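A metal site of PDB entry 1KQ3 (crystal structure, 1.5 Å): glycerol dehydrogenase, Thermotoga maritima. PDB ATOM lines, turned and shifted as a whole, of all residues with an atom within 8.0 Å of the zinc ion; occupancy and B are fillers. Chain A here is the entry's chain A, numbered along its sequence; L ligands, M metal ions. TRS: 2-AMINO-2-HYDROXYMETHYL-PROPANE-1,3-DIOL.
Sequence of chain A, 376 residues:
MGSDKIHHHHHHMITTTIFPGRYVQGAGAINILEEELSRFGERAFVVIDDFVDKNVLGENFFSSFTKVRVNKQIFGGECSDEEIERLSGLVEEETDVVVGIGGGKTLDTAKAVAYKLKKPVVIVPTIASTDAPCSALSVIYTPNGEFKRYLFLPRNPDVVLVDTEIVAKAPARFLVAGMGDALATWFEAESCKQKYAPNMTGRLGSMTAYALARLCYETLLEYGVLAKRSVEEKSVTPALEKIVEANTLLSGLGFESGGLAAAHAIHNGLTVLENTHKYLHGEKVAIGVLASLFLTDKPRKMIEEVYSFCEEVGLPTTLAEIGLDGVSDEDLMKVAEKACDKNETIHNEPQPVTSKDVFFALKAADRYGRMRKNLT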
ATOM      1  N   SER A 129     -20.731  14.373  -0.151  1.00  0.00           N
ATOM      2  CA  SER A 129     -20.009  15.546  -0.624  1.00  0.00           C
ATOM      3  C   SER A 129     -20.457  16.168  -1.930  1.00  0.00           C
ATOM      4  O   SER A 129     -19.953  17.238  -2.284  1.00  0.00           O
ATOM      5  CB  SER A 129     -18.511  15.236  -0.711  1.00  0.00           C
ATOM      6  OG  SER A 129     -18.306  14.222  -1.674  1.00  0.00           O
ATOM      7  N   THR A 130     -21.319  15.494  -2.682  1.00  0.00           N
ATOM      8  CA  THR A 130     -21.867  16.075  -3.927  1.00  0.00           C
ATOM      9  C   THR A 130     -23.239  15.492  -4.104  1.00  0.00           C
ATOM     10  O   THR A 130     -23.603  14.513  -3.443  1.00  0.00           O
ATOM     11  CB  THR A 130     -21.068  15.776  -5.246  1.00  0.00           C
ATOM     12  OG1 THR A 130     -21.352  14.462  -5.715  1.00  0.00           O
ATOM     13  CG2 THR A 130     -19.562  15.949  -5.036  1.00  0.00           C
ATOM     14  N   ASP A 131     -24.010  16.119  -4.981  1.00  0.00           N
ATOM     15  CA  ASP A 131     -25.362  15.643  -5.246  1.00  0.00           C
ATOM     16  C   ASP A 131     -25.457  14.754  -6.490  1.00  0.00           C
ATOM     17  O   ASP A 131     -26.539  14.552  -7.048  1.00  0.00           O
ATOM     18  CB  ASP A 131     -26.360  16.806  -5.314  1.00  0.00           C
ATOM     19  CG  ASP A 131     -25.983  17.850  -6.335  1.00  0.00           C
ATOM     20  OD1 ASP A 131     -25.076  17.619  -7.140  1.00  0.00           O
ATOM     21  OD2 ASP A 131     -26.619  18.914  -6.364  1.00  0.00           O
ATOM     22  N   ALA A 132     -24.341  14.182  -6.908  1.00  0.00           N
ATOM     23  CA  ALA A 132     -24.342  13.285  -8.045  1.00  0.00           C
ATOM     24  C   ALA A 132     -24.889  11.884  -7.879  1.00  0.00           C
ATOM     25  O   ALA A 132     -25.401  11.329  -8.838  1.00  0.00           O
ATOM     26  CB  ALA A 132     -22.922  13.147  -8.563  1.00  0.00           C
ATOM     27  N   ALA A 177     -18.514  20.338   2.156  1.00  0.00           N
ATOM     28  CA  ALA A 177     -18.445  20.532   0.702  1.00  0.00           C
ATOM     29  C   ALA A 177     -19.762  20.110   0.076  1.00  0.00           C
ATOM     30  O   ALA A 177     -20.205  20.747  -0.879  1.00  0.00           O
ATOM     31  CB  ALA A 177     -17.293  19.692   0.099  1.00  0.00           C
ATOM     32  N   GLY A 178     -20.387  19.026   0.586  1.00  0.00           N
ATOM     33  CA  GLY A 178     -21.694  18.612   0.057  1.00  0.00           C
ATOM     34  C   GLY A 178     -22.719  19.715   0.259  1.00  0.00           C
ATOM     35  O   GLY A 178     -23.592  19.917  -0.595  1.00  0.00           O
ATOM     36  N   GLY A 180     -22.060  22.843   0.172  1.00  0.00           N
ATOM     37  CA  GLY A 180     -21.746  23.866  -0.843  1.00  0.00           C
ATOM     38  C   GLY A 180     -22.371  23.500  -2.195  1.00  0.00           C
ATOM     39  O   GLY A 180     -22.942  24.377  -2.894  1.00  0.00           O
ATOM     40  N   ASP A 181     -22.255  22.233  -2.606  1.00  0.00           N
ATOM     41  CA  ASP A 181     -22.861  21.763  -3.858  1.00  0.00           C
ATOM     42  C   ASP A 181     -24.389  21.916  -3.741  1.00  0.00           C
ATOM     43  O   ASP A 181     -25.057  22.366  -4.702  1.00  0.00           O
ATOM     44  CB  ASP A 181     -22.427  20.299  -4.098  1.00  0.00           C
ATOM     45  CG  ASP A 181     -22.597  19.850  -5.543  1.00  0.00           C
ATOM     46  OD1 ASP A 181     -22.646  20.694  -6.462  1.00  0.00           O
ATOM     47  OD2 ASP A 181     -22.633  18.611  -5.743  1.00  0.00           O
ATOM     48  N   ALA A 182     -24.936  21.579  -2.575  1.00  0.00           N
ATOM     49  CA  ALA A 182     -26.369  21.684  -2.343  1.00  0.00           C
ATOM     50  C   ALA A 182     -26.896  23.112  -2.233  1.00  0.00           C
ATOM     51  O   ALA A 182     -28.047  23.370  -2.611  1.00  0.00           O
ATOM     52  CB  ALA A 182     -26.770  20.872  -1.064  1.00  0.00           C
ATOM     53  N   ALA A 184     -26.117  25.583  -3.974  1.00  0.00           N
ATOM     54  CA  ALA A 184     -26.375  26.106  -5.328  1.00  0.00           C
ATOM     55  C   ALA A 184     -27.717  25.678  -5.875  1.00  0.00           C
ATOM     56  O   ALA A 184     -28.269  26.354  -6.723  1.00  0.00           O
ATOM     57  CB  ALA A 184     -25.274  25.595  -6.286  1.00  0.00           C
ATOM     58  N   THR A 185     -28.257  24.570  -5.397  1.00  0.00           N
ATOM     59  CA  THR A 185     -29.433  23.975  -6.031  1.00  0.00           C
ATOM     60  C   THR A 185     -30.619  24.887  -6.178  1.00  0.00           C
ATOM     61  O   THR A 185     -31.164  25.013  -7.296  1.00  0.00           O
ATOM     62  CB  THR A 185     -29.777  22.704  -5.300  1.00  0.00           C
ATOM     63  OG1 THR A 185     -28.627  21.848  -5.389  1.00  0.00           O
ATOM     64  CG2 THR A 185     -30.952  21.985  -5.943  1.00  0.00           C
ATOM     65  N   GLU A 188     -29.881  27.973  -8.643  1.00  0.00           N
ATOM     66  CA  GLU A 188     -29.826  27.606 -10.052  1.00  0.00           C
ATOM     67  C   GLU A 188     -31.151  27.112 -10.571  1.00  0.00           C
ATOM     68  O   GLU A 188     -31.552  27.473 -11.696  1.00  0.00           O
ATOM     69  CB  GLU A 188     -28.730  26.558 -10.293  1.00  0.00           C
ATOM     70  CG  GLU A 188     -27.342  27.169 -10.074  1.00  0.00           C
ATOM     71  CD  GLU A 188     -26.182  26.232 -10.379  1.00  0.00           C
ATOM     72  OE1 GLU A 188     -25.662  26.268 -11.519  1.00  0.00           O
ATOM     73  OE2 GLU A 188     -25.767  25.493  -9.478  1.00  0.00           O
ATOM     74  N   SER A 251     -30.997  17.677  -3.263  1.00  0.00           N
ATOM     75  CA  SER A 251     -30.134  18.401  -4.184  1.00  0.00           C
ATOM     76  C   SER A 251     -30.007  17.674  -5.503  1.00  0.00           C
ATOM     77  O   SER A 251     -29.911  18.304  -6.538  1.00  0.00           O
ATOM     78  CB  SER A 251     -28.766  18.634  -3.539  1.00  0.00           C
ATOM     79  OG  SER A 251     -28.050  19.561  -4.342  1.00  0.00           O
ATOM     80  N   PHE A 255     -31.180  19.666  -8.822  1.00  0.00           N
ATOM     81  CA  PHE A 255     -30.323  20.116  -9.898  1.00  0.00           C
ATOM     82  C   PHE A 255     -30.646  19.412 -11.228  1.00  0.00           C
ATOM     83  O   PHE A 255     -30.663  20.029 -12.265  1.00  0.00           O
ATOM     84  CB  PHE A 255     -28.816  19.931  -9.536  1.00  0.00           C
ATOM     85  CG  PHE A 255     -28.175  18.689 -10.124  1.00  0.00           C
ATOM     86  CD1 PHE A 255     -27.798  18.654 -11.468  1.00  0.00           C
ATOM     87  CD2 PHE A 255     -27.948  17.559  -9.340  1.00  0.00           C
ATOM     88  CE1 PHE A 255     -27.224  17.508 -12.031  1.00  0.00           C
ATOM     89  CE2 PHE A 255     -27.371  16.416  -9.881  1.00  0.00           C
ATOM     90  CZ  PHE A 255     -27.002  16.380 -11.228  1.00  0.00           C
ATOM     91  N   LEU A 260     -29.488  23.631 -13.925  1.00  0.00           N
ATOM     92  CA  LEU A 260     -28.250  24.331 -13.547  1.00  0.00           C
ATOM     93  C   LEU A 260     -28.200  25.704 -14.201  1.00  0.00           C
ATOM     94  O   LEU A 260     -28.892  25.942 -15.205  1.00  0.00           O
ATOM     95  CB  LEU A 260     -27.042  23.500 -13.995  1.00  0.00           C
ATOM     96  CG  LEU A 260     -26.867  22.181 -13.236  1.00  0.00           C
ATOM     97  CD1 LEU A 260     -25.646  21.424 -13.779  1.00  0.00           C
ATOM     98  CD2 LEU A 260     -26.682  22.461 -11.766  1.00  0.00           C
ATOM     99  N   ALA A 263     -24.079  29.305 -10.980  1.00  0.00           N
ATOM    100  CA  ALA A 263     -23.087  28.796 -10.031  1.00  0.00           C
ATOM    101  C   ALA A 263     -22.213  27.701 -10.560  1.00  0.00           C
ATOM    102  O   ALA A 263     -20.995  27.731 -10.331  1.00  0.00           O
ATOM    103  CB  ALA A 263     -23.747  28.319  -8.737  1.00  0.00           C
ATOM    104  N   HIS A 264     -22.800  26.705 -11.206  1.00  0.00           N
ATOM    105  CA  HIS A 264     -21.941  25.628 -11.690  1.00  0.00           C
ATOM    106  C   HIS A 264     -21.077  26.075 -12.891  1.00  0.00           C
ATOM    107  O   HIS A 264     -19.957  25.560 -13.063  1.00  0.00           O
ATOM    108  CB  HIS A 264     -22.767  24.394 -12.018  1.00  0.00           C
ATOM    109  CG  HIS A 264     -22.915  23.463 -10.848  1.00  0.00           C
ATOM    110  ND1 HIS A 264     -23.727  23.740  -9.754  1.00  0.00           N
ATOM    111  CD2 HIS A 264     -22.265  22.309 -10.542  1.00  0.00           C
ATOM    112  CE1 HIS A 264     -23.572  22.794  -8.846  1.00  0.00           C
ATOM    113  NE2 HIS A 264     -22.696  21.917  -9.297  1.00  0.00           N
ATOM    114  N   HIS A 267     -18.164  27.636 -11.211  1.00  0.00           N
ATOM    115  CA  HIS A 267     -17.290  26.575 -10.700  1.00  0.00           C
ATOM    116  C   HIS A 267     -16.433  26.064 -11.854  1.00  0.00           C
ATOM    117  O   HIS A 267     -15.211  25.927 -11.700  1.00  0.00           O
ATOM    118  CB  HIS A 267     -18.106  25.374 -10.156  1.00  0.00           C
ATOM    119  CG  HIS A 267     -17.322  24.080 -10.112  1.00  0.00           C
ATOM    120  ND1 HIS A 267     -17.131  23.284 -11.215  1.00  0.00           N
ATOM    121  CD2 HIS A 267     -16.660  23.469  -9.091  1.00  0.00           C
ATOM    122  CE1 HIS A 267     -16.389  22.237 -10.889  1.00  0.00           C
ATOM    123  NE2 HIS A 267     -16.092  22.331  -9.604  1.00  0.00           N
ATOM    124  N   ASN A 268     -17.062  25.785 -13.010  1.00  0.00           N
ATOM    125  CA  ASN A 268     -16.302  25.255 -14.149  1.00  0.00           C
ATOM    126  C   ASN A 268     -15.241  26.236 -14.585  1.00  0.00           C
ATOM    127  O   ASN A 268     -14.128  25.801 -14.923  1.00  0.00           O
ATOM    128  CB  ASN A 268     -17.217  24.880 -15.305  1.00  0.00           C
ATOM    129  CG  ASN A 268     -18.072  23.708 -14.981  1.00  0.00           C
ATOM    130  OD1 ASN A 268     -17.874  23.052 -13.942  1.00  0.00           O
ATOM    131  ND2 ASN A 268     -19.028  23.407 -15.854  1.00  0.00           N
ATOM    132  N   HIS A 281     -15.143  20.060  -5.057  1.00  0.00           N
ATOM    133  CA  HIS A 281     -16.213  20.563  -5.923  1.00  0.00           C
ATOM    134  C   HIS A 281     -17.139  21.532  -5.196  1.00  0.00           C
ATOM    135  O   HIS A 281     -17.304  22.702  -5.615  1.00  0.00           O
ATOM    136  CB  HIS A 281     -17.049  19.389  -6.468  1.00  0.00           C
ATOM    137  CG  HIS A 281     -18.246  19.809  -7.275  1.00  0.00           C
ATOM    138  ND1 HIS A 281     -18.143  20.480  -8.475  1.00  0.00           N
ATOM    139  CD2 HIS A 281     -19.576  19.615  -7.072  1.00  0.00           C
ATOM    140  CE1 HIS A 281     -19.356  20.682  -8.980  1.00  0.00           C
ATOM    141  NE2 HIS A 281     -20.238  20.166  -8.146  1.00  0.00           N
ATOM    142  N   GLY A 282     -17.723  21.082  -4.086  1.00  0.00           N
ATOM    143  CA  GLY A 282     -18.680  21.917  -3.365  1.00  0.00           C
ATOM    144  C   GLY A 282     -18.113  23.185  -2.785  1.00  0.00           C
ATOM    145  O   GLY A 282     -18.839  24.166  -2.604  1.00  0.00           O
ATOM    146  N   VAL A 285     -18.072  25.425  -5.747  1.00  0.00           N
ATOM    147  CA  VAL A 285     -19.451  25.792  -6.122  1.00  0.00           C
ATOM    148  C   VAL A 285     -19.920  26.910  -5.179  1.00  0.00           C
ATOM    149  O   VAL A 285     -20.605  27.814  -5.621  1.00  0.00           O
ATOM    150  CB  VAL A 285     -20.397  24.563  -6.031  1.00  0.00           C
ATOM    151  CG1 VAL A 285     -21.865  24.990  -6.137  1.00  0.00           C
ATOM    152  CG2 VAL A 285     -20.130  23.612  -7.210  1.00  0.00           C
HETATM  153  C   TRS L   1     -23.176  18.179 -10.353  1.00  0.00           C
HETATM  154  C1  TRS L   1     -22.826  17.155  -9.175  1.00  0.00           C
HETATM  155  C2  TRS L   1     -24.549  18.818  -9.934  1.00  0.00           C
HETATM  156  C3  TRS L   1     -23.416  17.428 -11.668  1.00  0.00           C
HETATM  157  N   TRS L   1     -22.100  19.118 -10.423  1.00  0.00           N
HETATM  158  O1  TRS L   1     -22.083  17.969  -8.210  1.00  0.00           O
HETATM  159  O2  TRS L   1     -24.314  19.603  -8.711  1.00  0.00           O
HETATM  160  O3  TRS L   1     -22.207  16.733 -12.152  1.00  0.00           O
HETATM  161 ZN    ZN M   1     -22.282  20.080  -8.440  1.00  0.00          ZN
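A ring nitrogen (NE2) of His 267 lies within hydrogen-bond range of a ring nitrogen (ND1) of His 281, at 3.0 Å. The side-chain carboxylate (OE2) of Glu 188 sits at hydrogen-bond distance from a ring nitrogen (ND1) of His 264 (2.7 Å). OD1 of Asn 268 sits close to O of His 264 (3.4 Å). The side-chain carboxylate of Asp 181 is in hydrogen-bond range of the backbone NH of Asp 131 (2.9 Å). The side-chain carboxylate (OD2) of Asp 131 is in hydrogen-bond range of the side-chain hydroxyl (OG) of Ser 251.
Asp 131 touches the zinc ion. Of the 22 residues printed, 4 come within 4 Å of the zinc ion.
The zinc ion is bound by NE2 of His 281, 2.1 Å away. A ring nitrogen (NE2) of His 264 binds the zinc ion, at 2.1 Å. OD1 of Asp 181 binds the zinc ion, 2.1 Å away. The zinc ion is bound by O2 of the ligand. The zinc ion is bound by O1 of the ligand, 2.1 Å away. N of the ligand binds the zinc ion (2.2 Å).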
